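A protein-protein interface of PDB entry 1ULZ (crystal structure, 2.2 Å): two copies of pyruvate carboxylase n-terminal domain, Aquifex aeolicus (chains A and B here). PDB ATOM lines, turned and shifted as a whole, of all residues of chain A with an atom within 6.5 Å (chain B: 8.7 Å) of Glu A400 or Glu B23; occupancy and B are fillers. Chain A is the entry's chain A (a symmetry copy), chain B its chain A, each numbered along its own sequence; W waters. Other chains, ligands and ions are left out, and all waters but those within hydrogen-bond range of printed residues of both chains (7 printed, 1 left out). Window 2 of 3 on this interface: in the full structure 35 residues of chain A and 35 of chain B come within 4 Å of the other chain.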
ATOM      1  N   ILE A 334     -16.252   8.355  15.679  1.00  0.00           N
ATOM      2  CA  ILE A 334     -15.230   7.333  15.557  1.00  0.00           C
ATOM      3  C   ILE A 334     -14.859   7.174  14.094  1.00  0.00           C
ATOM      4  O   ILE A 334     -15.724   7.242  13.223  1.00  0.00           O
ATOM      5  CB  ILE A 334     -15.733   5.970  16.059  1.00  0.00           C
ATOM      6  CG1 ILE A 334     -16.222   6.086  17.505  1.00  0.00           C
ATOM      7  CG2 ILE A 334     -14.621   4.943  15.936  1.00  0.00           C
ATOM      8  CD1 ILE A 334     -16.941   4.855  18.010  1.00  0.00           C
ATOM      9  N   PHE A 363     -28.062   7.925   8.866  1.00  0.00           N
ATOM     10  CA  PHE A 363     -27.963   8.926   9.921  1.00  0.00           C
ATOM     11  C   PHE A 363     -26.656   8.741  10.712  1.00  0.00           C
ATOM     12  O   PHE A 363     -26.377   7.652  11.219  1.00  0.00           O
ATOM     13  CB  PHE A 363     -29.182   8.778  10.842  1.00  0.00           C
ATOM     14  CG  PHE A 363     -29.243   9.780  11.967  1.00  0.00           C
ATOM     15  CD1 PHE A 363     -28.255   9.827  12.938  1.00  0.00           C
ATOM     16  CD2 PHE A 363     -30.323  10.643  12.077  1.00  0.00           C
ATOM     17  CE1 PHE A 363     -28.343  10.712  13.998  1.00  0.00           C
ATOM     18  CE2 PHE A 363     -30.419  11.530  13.134  1.00  0.00           C
ATOM     19  CZ  PHE A 363     -29.431  11.567  14.096  1.00  0.00           C
ATOM     20  N   ILE A 365     -23.597   8.746   9.574  1.00  0.00           N
ATOM     21  CA  ILE A 365     -22.553   8.045   8.842  1.00  0.00           C
ATOM     22  C   ILE A 365     -21.919   8.923   7.773  1.00  0.00           C
ATOM     23  O   ILE A 365     -22.619   9.553   6.980  1.00  0.00           O
ATOM     24  CB  ILE A 365     -23.108   6.772   8.157  1.00  0.00           C
ATOM     25  CG1 ILE A 365     -23.603   5.784   9.217  1.00  0.00           C
ATOM     26  CG2 ILE A 365     -22.034   6.140   7.266  1.00  0.00           C
ATOM     27  CD1 ILE A 365     -24.228   4.547   8.621  1.00  0.00           C
ATOM     28  N   TRP A 395     -21.016   7.515  23.679  1.00  0.00           N
ATOM     29  CA  TRP A 395     -19.969   6.579  23.304  1.00  0.00           C
ATOM     30  C   TRP A 395     -20.480   5.215  22.847  1.00  0.00           C
ATOM     31  O   TRP A 395     -20.068   4.721  21.801  1.00  0.00           O
ATOM     32  CB  TRP A 395     -18.996   6.380  24.467  1.00  0.00           C
ATOM     33  CG  TRP A 395     -18.014   5.287  24.217  1.00  0.00           C
ATOM     34  CD1 TRP A 395     -17.945   4.083  24.858  1.00  0.00           C
ATOM     35  CD2 TRP A 395     -16.970   5.281  23.234  1.00  0.00           C
ATOM     36  NE1 TRP A 395     -16.921   3.329  24.336  1.00  0.00           N
ATOM     37  CE2 TRP A 395     -16.307   4.041  23.337  1.00  0.00           C
ATOM     38  CE3 TRP A 395     -16.531   6.203  22.275  1.00  0.00           C
ATOM     39  CZ2 TRP A 395     -15.230   3.699  22.520  1.00  0.00           C
ATOM     40  CZ3 TRP A 395     -15.464   5.863  21.465  1.00  0.00           C
ATOM     41  CH2 TRP A 395     -14.825   4.620  21.594  1.00  0.00           C
ATOM     42  N   ASP A 396     -21.371   4.599  23.617  1.00  0.00           N
ATOM     43  CA  ASP A 396     -21.851   3.280  23.224  1.00  0.00           C
ATOM     44  C   ASP A 396     -22.649   3.288  21.930  1.00  0.00           C
ATOM     45  O   ASP A 396     -22.554   2.348  21.140  1.00  0.00           O
ATOM     46  CB  ASP A 396     -22.676   2.622  24.333  1.00  0.00           C
ATOM     47  CG  ASP A 396     -22.931   1.147  24.053  1.00  0.00           C
ATOM     48  OD1 ASP A 396     -24.050   0.791  23.614  1.00  0.00           O
ATOM     49  OD2 ASP A 396     -21.992   0.342  24.249  1.00  0.00           O
ATOM     50  N   GLU A 397     -23.425   4.346  21.702  1.00  0.00           N
ATOM     51  CA  GLU A 397     -24.206   4.447  20.476  1.00  0.00           C
ATOM     52  C   GLU A 397     -23.290   4.611  19.268  1.00  0.00           C
ATOM     53  O   GLU A 397     -23.578   4.100  18.189  1.00  0.00           O
ATOM     54  CB  GLU A 397     -25.160   5.628  20.545  1.00  0.00           C
ATOM     55  CG  GLU A 397     -26.136   5.549  21.687  1.00  0.00           C
ATOM     56  CD  GLU A 397     -27.139   6.670  21.654  1.00  0.00           C
ATOM     57  OE1 GLU A 397     -28.163   6.533  20.955  1.00  0.00           O
ATOM     58  OE2 GLU A 397     -26.895   7.699  22.310  1.00  0.00           O
ATOM     59  N   ALA A 398     -22.188   5.329  19.458  1.00  0.00           N
ATOM     60  CA  ALA A 398     -21.231   5.556  18.381  1.00  0.00           C
ATOM     61  C   ALA A 398     -20.554   4.236  18.034  1.00  0.00           C
ATOM     62  O   ALA A 398     -20.311   3.940  16.863  1.00  0.00           O
ATOM     63  CB  ALA A 398     -20.196   6.586  18.811  1.00  0.00           C
ATOM     64  N   VAL A 399     -20.254   3.445  19.060  1.00  0.00           N
ATOM     65  CA  VAL A 399     -19.621   2.148  18.859  1.00  0.00           C
ATOM     66  C   VAL A 399     -20.548   1.233  18.060  1.00  0.00           C
ATOM     67  O   VAL A 399     -20.130   0.604  17.089  1.00  0.00           O
ATOM     68  CB  VAL A 399     -19.290   1.470  20.208  1.00  0.00           C
ATOM     69  CG1 VAL A 399     -18.724   0.075  19.971  1.00  0.00           C
ATOM     70  CG2 VAL A 399     -18.293   2.331  20.988  1.00  0.00           C
ATOM     71  N   GLU A 400     -21.809   1.163  18.477  1.00  0.00           N
ATOM     72  CA  GLU A 400     -22.786   0.326  17.793  1.00  0.00           C
ATOM     73  C   GLU A 400     -23.061   0.822  16.378  1.00  0.00           C
ATOM     74  O   GLU A 400     -23.285   0.016  15.475  1.00  0.00           O
ATOM     75  CB  GLU A 400     -24.088   0.255  18.599  1.00  0.00           C
ATOM     76  CG  GLU A 400     -23.922  -0.457  19.937  1.00  0.00           C
ATOM     77  CD  GLU A 400     -23.279  -1.836  19.801  1.00  0.00           C
ATOM     78  OE1 GLU A 400     -22.396  -2.165  20.625  1.00  0.00           O
ATOM     79  OE2 GLU A 400     -23.654  -2.597  18.880  1.00  0.00           O
ATOM     80  N   ARG A 401     -23.041   2.139  16.175  1.00  0.00           N
ATOM     81  CA  ARG A 401     -23.270   2.672  14.833  1.00  0.00           C
ATOM     82  C   ARG A 401     -22.120   2.247  13.924  1.00  0.00           C
ATOM     83  O   ARG A 401     -22.343   1.838  12.785  1.00  0.00           O
ATOM     84  CB  ARG A 401     -23.358   4.197  14.836  1.00  0.00           C
ATOM     85  CG  ARG A 401     -23.629   4.794  13.453  1.00  0.00           C
ATOM     86  CD  ARG A 401     -25.060   5.347  13.360  1.00  0.00           C
ATOM     87  NE  ARG A 401     -25.163   6.629  14.031  1.00  0.00           N
ATOM     88  CZ  ARG A 401     -26.285   7.168  14.497  1.00  0.00           C
ATOM     89  NH1 ARG A 401     -26.227   8.352  15.089  1.00  0.00           N
ATOM     90  NH2 ARG A 401     -27.450   6.536  14.392  1.00  0.00           N
ATOM     91  N   MET A 402     -20.891   2.342  14.432  1.00  0.00           N
ATOM     92  CA  MET A 402     -19.726   1.952  13.648  1.00  0.00           C
ATOM     93  C   MET A 402     -19.794   0.472  13.269  1.00  0.00           C
ATOM     94  O   MET A 402     -19.634   0.120  12.104  1.00  0.00           O
ATOM     95  CB  MET A 402     -18.436   2.228  14.424  1.00  0.00           C
ATOM     96  CG  MET A 402     -17.166   1.856  13.672  1.00  0.00           C
ATOM     97  SD  MET A 402     -17.033   2.683  12.060  1.00  0.00           S
ATOM     98  CE  MET A 402     -16.224   4.188  12.499  1.00  0.00           C
ATOM     99  N   ARG A 403     -20.040  -0.396  14.249  1.00  0.00           N
ATOM    100  CA  ARG A 403     -20.116  -1.830  13.975  1.00  0.00           C
ATOM    101  C   ARG A 403     -21.182  -2.161  12.927  1.00  0.00           C
ATOM    102  O   ARG A 403     -20.953  -2.992  12.048  1.00  0.00           O
ATOM    103  CB  ARG A 403     -20.394  -2.618  15.260  1.00  0.00           C
ATOM    104  CG  ARG A 403     -20.458  -4.123  15.026  1.00  0.00           C
ATOM    105  CD  ARG A 403     -20.294  -4.911  16.312  1.00  0.00           C
ATOM    106  NE  ARG A 403     -21.439  -4.799  17.211  1.00  0.00           N
ATOM    107  CZ  ARG A 403     -22.546  -5.529  17.106  1.00  0.00           C
ATOM    108  NH1 ARG A 403     -22.664  -6.428  16.137  1.00  0.00           N
ATOM    109  NH2 ARG A 403     -23.532  -5.370  17.981  1.00  0.00           N
ATOM    110  N   ALA A 404     -22.335  -1.498  13.020  1.00  0.00           N
ATOM    111  CA  ALA A 404     -23.434  -1.715  12.078  1.00  0.00           C
ATOM    112  C   ALA A 404     -23.042  -1.259  10.673  1.00  0.00           C
ATOM    113  O   ALA A 404     -23.406  -1.885   9.686  1.00  0.00           O
ATOM    114  CB  ALA A 404     -24.694  -0.975  12.546  1.00  0.00           C
ATOM    115  N   ALA A 405     -22.301  -0.162  10.588  1.00  0.00           N
ATOM    116  CA  ALA A 405     -21.850   0.351   9.299  1.00  0.00           C
ATOM    117  C   ALA A 405     -20.817  -0.619   8.712  1.00  0.00           C
ATOM    118  O   ALA A 405     -20.894  -0.986   7.541  1.00  0.00           O
ATOM    119  CB  ALA A 405     -21.240   1.740   9.472  1.00  0.00           C
ATOM    120  N   MET A 425     -14.917  -3.444  17.752  1.00  0.00           N
ATOM    121  CA  MET A 425     -16.165  -2.812  18.170  1.00  0.00           C
ATOM    122  C   MET A 425     -16.953  -3.719  19.113  1.00  0.00           C
ATOM    123  O   MET A 425     -17.741  -3.235  19.922  1.00  0.00           O
ATOM    124  CB  MET A 425     -17.043  -2.474  16.953  1.00  0.00           C
ATOM    125  CG  MET A 425     -16.431  -1.505  15.951  1.00  0.00           C
ATOM    126  SD  MET A 425     -16.067   0.099  16.674  1.00  0.00           S
ATOM    127  CE  MET A 425     -14.313   0.262  16.303  1.00  0.00           C
ATOM    128  N   LYS A 426     -16.745  -5.031  18.999  1.00  0.00           N
ATOM    129  CA  LYS A 426     -17.437  -6.004  19.852  1.00  0.00           C
ATOM    130  C   LYS A 426     -16.674  -6.301  21.136  1.00  0.00           C
ATOM    131  O   LYS A 426     -17.236  -6.851  22.083  1.00  0.00           O
ATOM    132  CB  LYS A 426     -17.620  -7.344  19.133  1.00  0.00           C
ATOM    133  CG  LYS A 426     -18.570  -7.362  17.967  1.00  0.00           C
ATOM    134  CD  LYS A 426     -18.651  -8.776  17.404  1.00  0.00           C
ATOM    135  CE  LYS A 426     -19.634  -8.858  16.247  1.00  0.00           C
ATOM    136  NZ  LYS A 426     -19.636 -10.222  15.652  1.00  0.00           N
ATOM    137  N   LYS A 431     -15.558  -1.388  24.171  1.00  0.00           N
ATOM    138  CA  LYS A 431     -16.927  -0.946  24.415  1.00  0.00           C
ATOM    139  C   LYS A 431     -17.022  -0.148  25.701  1.00  0.00           C
ATOM    140  O   LYS A 431     -17.773   0.827  25.784  1.00  0.00           O
ATOM    141  CB  LYS A 431     -17.878  -2.138  24.498  1.00  0.00           C
ATOM    142  CG  LYS A 431     -18.020  -2.898  23.202  1.00  0.00           C
ATOM    143  CD  LYS A 431     -19.338  -3.637  23.188  1.00  0.00           C
ATOM    144  CE  LYS A 431     -20.467  -2.647  23.435  1.00  0.00           C
ATOM    145  NZ  LYS A 431     -21.798  -3.239  23.153  1.00  0.00           N
ATOM    146  N   VAL B  15     -33.237  -1.067   3.767  1.00  0.00           N
ATOM    147  CA  VAL B  15     -31.872  -0.890   4.260  1.00  0.00           C
ATOM    148  C   VAL B  15     -31.878   0.085   5.438  1.00  0.00           C
ATOM    149  O   VAL B  15     -31.226  -0.153   6.450  1.00  0.00           O
ATOM    150  CB  VAL B  15     -30.944  -0.346   3.147  1.00  0.00           C
ATOM    151  CG1 VAL B  15     -29.606   0.075   3.740  1.00  0.00           C
ATOM    152  CG2 VAL B  15     -30.732  -1.416   2.077  1.00  0.00           C
ATOM    153  N   ARG B  16     -32.627   1.177   5.296  1.00  0.00           N
ATOM    154  CA  ARG B  16     -32.753   2.187   6.345  1.00  0.00           C
ATOM    155  C   ARG B  16     -33.284   1.557   7.628  1.00  0.00           C
ATOM    156  O   ARG B  16     -32.745   1.781   8.706  1.00  0.00           O
ATOM    157  CB  ARG B  16     -33.714   3.294   5.905  1.00  0.00           C
ATOM    158  CG  ARG B  16     -34.059   4.311   7.001  1.00  0.00           C
ATOM    159  CD  ARG B  16     -32.942   5.327   7.200  1.00  0.00           C
ATOM    160  NE  ARG B  16     -33.216   6.279   8.275  1.00  0.00           N
ATOM    161  CZ  ARG B  16     -33.053   6.020   9.571  1.00  0.00           C
ATOM    162  NH1 ARG B  16     -32.616   4.830   9.970  1.00  0.00           N
ATOM    163  NH2 ARG B  16     -33.312   6.959  10.470  1.00  0.00           N
ATOM    164  N   ILE B  17     -34.349   0.770   7.502  1.00  0.00           N
ATOM    165  CA  ILE B  17     -34.955   0.108   8.651  1.00  0.00           C
ATOM    166  C   ILE B  17     -34.005  -0.925   9.263  1.00  0.00           C
ATOM    167  O   ILE B  17     -33.861  -0.994  10.484  1.00  0.00           O
ATOM    168  CB  ILE B  17     -36.286  -0.584   8.263  1.00  0.00           C
ATOM    169  CG1 ILE B  17     -37.276   0.461   7.735  1.00  0.00           C
ATOM    170  CG2 ILE B  17     -36.878  -1.302   9.476  1.00  0.00           C
ATOM    171  CD1 ILE B  17     -38.511  -0.124   7.108  1.00  0.00           C
ATOM    172  N   ILE B  18     -33.357  -1.724   8.419  1.00  0.00           N
ATOM    173  CA  ILE B  18     -32.423  -2.732   8.912  1.00  0.00           C
ATOM    174  C   ILE B  18     -31.278  -2.087   9.698  1.00  0.00           C
ATOM    175  O   ILE B  18     -30.876  -2.596  10.741  1.00  0.00           O
ATOM    176  CB  ILE B  18     -31.839  -3.586   7.754  1.00  0.00           C
ATOM    177  CG1 ILE B  18     -32.894  -4.579   7.261  1.00  0.00           C
ATOM    178  CG2 ILE B  18     -30.603  -4.342   8.220  1.00  0.00           C
ATOM    179  CD1 ILE B  18     -32.463  -5.381   6.057  1.00  0.00           C
ATOM    180  N   ARG B  19     -30.764  -0.960   9.216  1.00  0.00           N
ATOM    181  CA  ARG B  19     -29.671  -0.298   9.923  1.00  0.00           C
ATOM    182  C   ARG B  19     -30.112   0.156  11.315  1.00  0.00           C
ATOM    183  O   ARG B  19     -29.377  -0.002  12.290  1.00  0.00           O
ATOM    184  CB  ARG B  19     -29.146   0.910   9.133  1.00  0.00           C
ATOM    185  CG  ARG B  19     -28.004   1.625   9.850  1.00  0.00           C
ATOM    186  CD  ARG B  19     -27.330   2.673   8.990  1.00  0.00           C
ATOM    187  NE  ARG B  19     -26.793   2.118   7.754  1.00  0.00           N
ATOM    188  CZ  ARG B  19     -25.893   1.141   7.693  1.00  0.00           C
ATOM    189  NH1 ARG B  19     -25.418   0.594   8.803  1.00  0.00           N
ATOM    190  NH2 ARG B  19     -25.462   0.714   6.518  1.00  0.00           N
ATOM    191  N   ALA B  20     -31.308   0.731  11.403  1.00  0.00           N
ATOM    192  CA  ALA B  20     -31.828   1.184  12.691  1.00  0.00           C
ATOM    193  C   ALA B  20     -31.874  -0.008  13.649  1.00  0.00           C
ATOM    194  O   ALA B  20     -31.416   0.087  14.788  1.00  0.00           O
ATOM    195  CB  ALA B  20     -33.220   1.787  12.517  1.00  0.00           C
ATOM    196  N   CYS B  21     -32.417  -1.129  13.176  1.00  0.00           N
ATOM    197  CA  CYS B  21     -32.507  -2.347  13.979  1.00  0.00           C
ATOM    198  C   CYS B  21     -31.134  -2.850  14.432  1.00  0.00           C
ATOM    199  O   CYS B  21     -30.949  -3.189  15.598  1.00  0.00           O
ATOM    200  CB  CYS B  21     -33.228  -3.454  13.194  1.00  0.00           C
ATOM    201  SG  CYS B  21     -35.010  -3.177  12.951  1.00  0.00           S
ATOM    202  N   LYS B  22     -30.174  -2.899  13.510  1.00  0.00           N
ATOM    203  CA  LYS B  22     -28.827  -3.356  13.839  1.00  0.00           C
ATOM    204  C   LYS B  22     -28.233  -2.482  14.936  1.00  0.00           C
ATOM    205  O   LYS B  22     -27.573  -2.977  15.847  1.00  0.00           O
ATOM    206  CB  LYS B  22     -27.921  -3.328  12.599  1.00  0.00           C
ATOM    207  CG  LYS B  22     -28.257  -4.385  11.556  1.00  0.00           C
ATOM    208  CD  LYS B  22     -27.317  -4.312  10.355  1.00  0.00           C
ATOM    209  CE  LYS B  22     -25.881  -4.672  10.717  1.00  0.00           C
ATOM    210  NZ  LYS B  22     -25.707  -6.123  10.997  1.00  0.00           N
ATOM    211  N   GLU B  23     -28.475  -1.179  14.848  1.00  0.00           N
ATOM    212  CA  GLU B  23     -27.970  -0.259  15.855  1.00  0.00           C
ATOM    213  C   GLU B  23     -28.610  -0.537  17.220  1.00  0.00           C
ATOM    214  O   GLU B  23     -27.967  -0.371  18.254  1.00  0.00           O
ATOM    215  CB  GLU B  23     -28.205   1.190  15.411  1.00  0.00           C
ATOM    216  CG  GLU B  23     -27.132   1.679  14.449  1.00  0.00           C
ATOM    217  CD  GLU B  23     -27.440   3.023  13.803  1.00  0.00           C
ATOM    218  OE1 GLU B  23     -28.257   3.796  14.348  1.00  0.00           O
ATOM    219  OE2 GLU B  23     -26.842   3.310  12.745  1.00  0.00           O
ATOM    220  N   LEU B  24     -29.865  -0.980  17.220  1.00  0.00           N
ATOM    221  CA  LEU B  24     -30.557  -1.288  18.469  1.00  0.00           C
ATOM    222  C   LEU B  24     -30.219  -2.704  18.936  1.00  0.00           C
ATOM    223  O   LEU B  24     -30.548  -3.089  20.053  1.00  0.00           O
ATOM    224  CB  LEU B  24     -32.077  -1.155  18.303  1.00  0.00           C
ATOM    225  CG  LEU B  24     -32.652   0.249  18.068  1.00  0.00           C
ATOM    226  CD1 LEU B  24     -34.120   0.154  17.704  1.00  0.00           C
ATOM    227  CD2 LEU B  24     -32.474   1.103  19.312  1.00  0.00           C
ATOM    228  N   GLY B  25     -29.554  -3.474  18.079  1.00  0.00           N
ATOM    229  CA  GLY B  25     -29.202  -4.838  18.437  1.00  0.00           C
ATOM    230  C   GLY B  25     -30.382  -5.780  18.270  1.00  0.00           C
ATOM    231  O   GLY B  25     -30.484  -6.796  18.955  1.00  0.00           O
ATOM    232  N   ILE B  26     -31.285  -5.435  17.357  1.00  0.00           N
ATOM    233  CA  ILE B  26     -32.473  -6.239  17.096  1.00  0.00           C
ATOM    234  C   ILE B  26     -32.308  -7.051  15.814  1.00  0.00           C
ATOM    235  O   ILE B  26     -32.084  -6.486  14.742  1.00  0.00           O
ATOM    236  CB  ILE B  26     -33.723  -5.344  16.944  1.00  0.00           C
ATOM    237  CG1 ILE B  26     -33.990  -4.598  18.254  1.00  0.00           C
ATOM    238  CG2 ILE B  26     -34.931  -6.189  16.547  1.00  0.00           C
ATOM    239  CD1 ILE B  26     -35.129  -3.608  18.171  1.00  0.00           C
ATOM    240  N   PRO B  27     -32.406  -8.389  15.912  1.00  0.00           N
ATOM    241  CA  PRO B  27     -32.263  -9.239  14.727  1.00  0.00           C
ATOM    242  C   PRO B  27     -33.343  -8.885  13.716  1.00  0.00           C
ATOM    243  O   PRO B  27     -34.448  -8.490  14.094  1.00  0.00           O
ATOM    244  CB  PRO B  27     -32.416 -10.656  15.291  1.00  0.00           C
ATOM    245  CG  PRO B  27     -33.311 -10.461  16.468  1.00  0.00           C
ATOM    246  CD  PRO B  27     -32.759  -9.191  17.096  1.00  0.00           C
ATOM    247  N   THR B  28     -33.030  -9.027  12.434  1.00  0.00           N
ATOM    248  CA  THR B  28     -33.992  -8.684  11.397  1.00  0.00           C
ATOM    249  C   THR B  28     -34.314  -9.815  10.441  1.00  0.00           C
ATOM    250  O   THR B  28     -33.534 -10.760  10.282  1.00  0.00           O
ATOM    251  CB  THR B  28     -33.492  -7.501  10.551  1.00  0.00           C
ATOM    252  OG1 THR B  28     -32.272  -7.863   9.897  1.00  0.00           O
ATOM    253  CG2 THR B  28     -33.246  -6.294  11.430  1.00  0.00           C
ATOM    254  N   ASP B 306     -33.327  10.874  15.188  1.00  0.00           N
ATOM    255  CA  ASP B 306     -33.445   9.673  14.365  1.00  0.00           C
ATOM    256  C   ASP B 306     -34.896   9.177  14.414  1.00  0.00           C
ATOM    257  O   ASP B 306     -35.329   8.526  15.373  1.00  0.00           O
ATOM    258  CB  ASP B 306     -32.464   8.616  14.886  1.00  0.00           C
ATOM    259  CG  ASP B 306     -32.393   7.382  13.999  1.00  0.00           C
ATOM    260  OD1 ASP B 306     -31.318   6.747  13.968  1.00  0.00           O
ATOM    261  OD2 ASP B 306     -33.406   7.035  13.355  1.00  0.00           O
ATOM    262  N   VAL B 308     -36.656   6.932  12.331  1.00  0.00           N
ATOM    263  CA  VAL B 308     -36.898   5.499  12.190  1.00  0.00           C
ATOM    264  C   VAL B 308     -36.588   4.717  13.464  1.00  0.00           C
ATOM    265  O   VAL B 308     -37.350   3.831  13.849  1.00  0.00           O
ATOM    266  CB  VAL B 308     -36.092   4.904  11.027  1.00  0.00           C
ATOM    267  CG1 VAL B 308     -36.272   3.391  10.995  1.00  0.00           C
ATOM    268  CG2 VAL B 308     -36.559   5.521   9.710  1.00  0.00           C
ATOM    269  N   LYS B 309     -35.474   5.041  14.118  1.00  0.00           N
ATOM    270  CA  LYS B 309     -35.118   4.356  15.354  1.00  0.00           C
ATOM    271  C   LYS B 309     -36.206   4.621  16.392  1.00  0.00           C
ATOM    272  O   LYS B 309     -36.593   3.724  17.135  1.00  0.00           O
ATOM    273  CB  LYS B 309     -33.757   4.831  15.883  1.00  0.00           C
ATOM    274  CG  LYS B 309     -33.305   4.078  17.141  1.00  0.00           C
ATOM    275  CD  LYS B 309     -31.878   4.432  17.552  1.00  0.00           C
ATOM    276  CE  LYS B 309     -30.862   3.957  16.513  1.00  0.00           C
ATOM    277  NZ  LYS B 309     -29.476   4.363  16.852  1.00  0.00           N
ATOM    278  N   ILE B 312     -39.329   2.415  16.140  1.00  0.00           N
ATOM    279  CA  ILE B 312     -39.175   1.112  16.773  1.00  0.00           C
ATOM    280  C   ILE B 312     -39.256   1.187  18.294  1.00  0.00           C
ATOM    281  O   ILE B 312     -39.927   0.368  18.918  1.00  0.00           O
ATOM    282  CB  ILE B 312     -37.850   0.450  16.344  1.00  0.00           C
ATOM    283  CG1 ILE B 312     -37.821   0.326  14.810  1.00  0.00           C
ATOM    284  CG2 ILE B 312     -37.734  -0.928  16.968  1.00  0.00           C
ATOM    285  CD1 ILE B 312     -36.458   0.033  14.224  1.00  0.00           C
ATOM    286  N   LYS B 313     -38.585   2.169  18.886  1.00  0.00           N
ATOM    287  CA  LYS B 313     -38.622   2.332  20.336  1.00  0.00           C
ATOM    288  C   LYS B 313     -40.059   2.591  20.789  1.00  0.00           C
ATOM    289  O   LYS B 313     -40.512   2.045  21.790  1.00  0.00           O
ATOM    290  CB  LYS B 313     -37.724   3.496  20.769  1.00  0.00           C
ATOM    291  CG  LYS B 313     -36.244   3.252  20.527  1.00  0.00           C
ATOM    292  CD  LYS B 313     -35.379   4.405  21.019  1.00  0.00           C
ATOM    293  CE  LYS B 313     -33.899   4.036  20.896  1.00  0.00           C
ATOM    294  NZ  LYS B 313     -32.961   5.145  21.266  1.00  0.00           N
HETATM  295  O   HOH W   1     -24.795   1.976  11.227  1.00  0.00           O
HETATM  296  O   HOH W   2     -24.172  -2.737  15.906  1.00  0.00           O
HETATM  297  O   HOH W   3     -27.738   6.302  18.070  1.00  0.00           O
HETATM  298  O   HOH W   4     -26.160   4.160  17.653  1.00  0.00           O
HETATM  299  O   HOH W   5     -29.561   5.582   9.171  1.00  0.00           O
HETATM  300  O   HOH W   6     -30.037   7.256  16.311  1.00  0.00           O
HETATM  301  O   HOH W   7     -27.844   5.320  11.091  1.00  0.00           O
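The backbone carbonyl oxygen (O) of Ala A404 sits at hydrogen-bond distance from the guanidinium group (NH1) of Arg B19, 3.3 Å away.
NH2 of Arg A401 lies within salt-bridge range of OE1 of Glu B23, at 2.9 Å.
The guanidinium group (NH2) of Arg A401 is in salt-bridge range of the side-chain carboxylate (OD1) of Asp B306, at 3.9 Å.
OD2 of Asp B306 lies within salt-bridge range of NH2 of Arg B16 (2.9 Å).
OE1 of Glu B23 lies within salt-bridge range of NZ of Lys B309, 2.8 Å away.
The side-chain carboxylate (OD2) of Asp B306 is in hydrogen-bond range of the backbone NH (N) of Lys B309 (3.0 Å).
O of Phe A363 lies within hydrogen-bond range of NE of Arg A401, 3.2 Å away.
The guanidinium group (NH2) of Arg A403 lies within salt-bridge range of the side-chain carboxylate (OE2) of Glu A400.
The side-chain carboxylate (OE1) of Glu A400 lies within salt-bridge range of the side-chain amino group (NZ) of Lys A431 (2.8 Å).
Among the printed residues, pairs that only touch across the chains: Phe A363 with Asp B306, Ile A365 with Arg B19, Glu A400 with Glu B23, Arg A401 with Lys B309, Ala A404 with Lys B22 and Ala A405 with Arg B19.
Printed residues of chain B within 4 Å of Ile A365: Arg B19 (3.6 Å).
Of chain B, only Glu B23 (3.9 Å) comes within 4 Å of Glu A400.
Lys A426 touches none of the printed residues of chain B.
Of the printed residues of chain A, Arg B19 touches Ile A365 (3.6 Å), Ala A404 (3.3 Å) and Ala A405 (3.6 Å).
Cys B21 touches none of the printed residues of chain A.
Of chain A, only Glu A400 (3.9 Å) and Arg A401 (2.8 Å) come within 4 Å of Glu B23.
The nearest residue of chain B that does not touch Glu A400 is Lys B22 (5.0 Å).
Hydrophobic or aromatic side chains of chain A that line the printed part of chain B: Phe A363, Ile A365 and Ala A404.
No position is printed for both chains.
Of the 9 pairs that touch across the chains among the printed residues, none has its exchanged pair printed and touching as well.
Water W6 lies within hydrogen-bond range of the side-chain carboxylate (OD1) of Asp B306 (2.7 Å), the side-chain amino group (NZ) of Lys B309 (3.0 Å) and the guanidinium group (NH2) of Arg A401 (3.3 Å).
Water W7 lies within hydrogen-bond range of the backbone carbonyl oxygen of Phe A363 (2.8 Å) and the side-chain carboxylate of Glu B23 (2.8 Å).
Water W5 bridges N of Phe A363 (2.8 Å) and NH1 of Arg B16 (3.2 Å).
Water W1 lies within hydrogen-bond range of the guanidinium group (NH1) of Arg B19 (2.9 Å), the side-chain carboxylate (OE2) of Glu B23 (2.9 Å), the backbone carbonyl oxygen (O) of Arg A401 (2.9 Å) and the backbone NH (N) of Ala A405 (3.3 Å).
Water W3 bridges NZ of Lys B309 (2.9 Å) and OE1 of Glu A397 (2.9 Å).
Water W2 lies within hydrogen-bond range of O of Glu A400 (2.9 Å), O of Lys B22 (3.4 Å) and NH2 of Arg A403 (3.4 Å).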
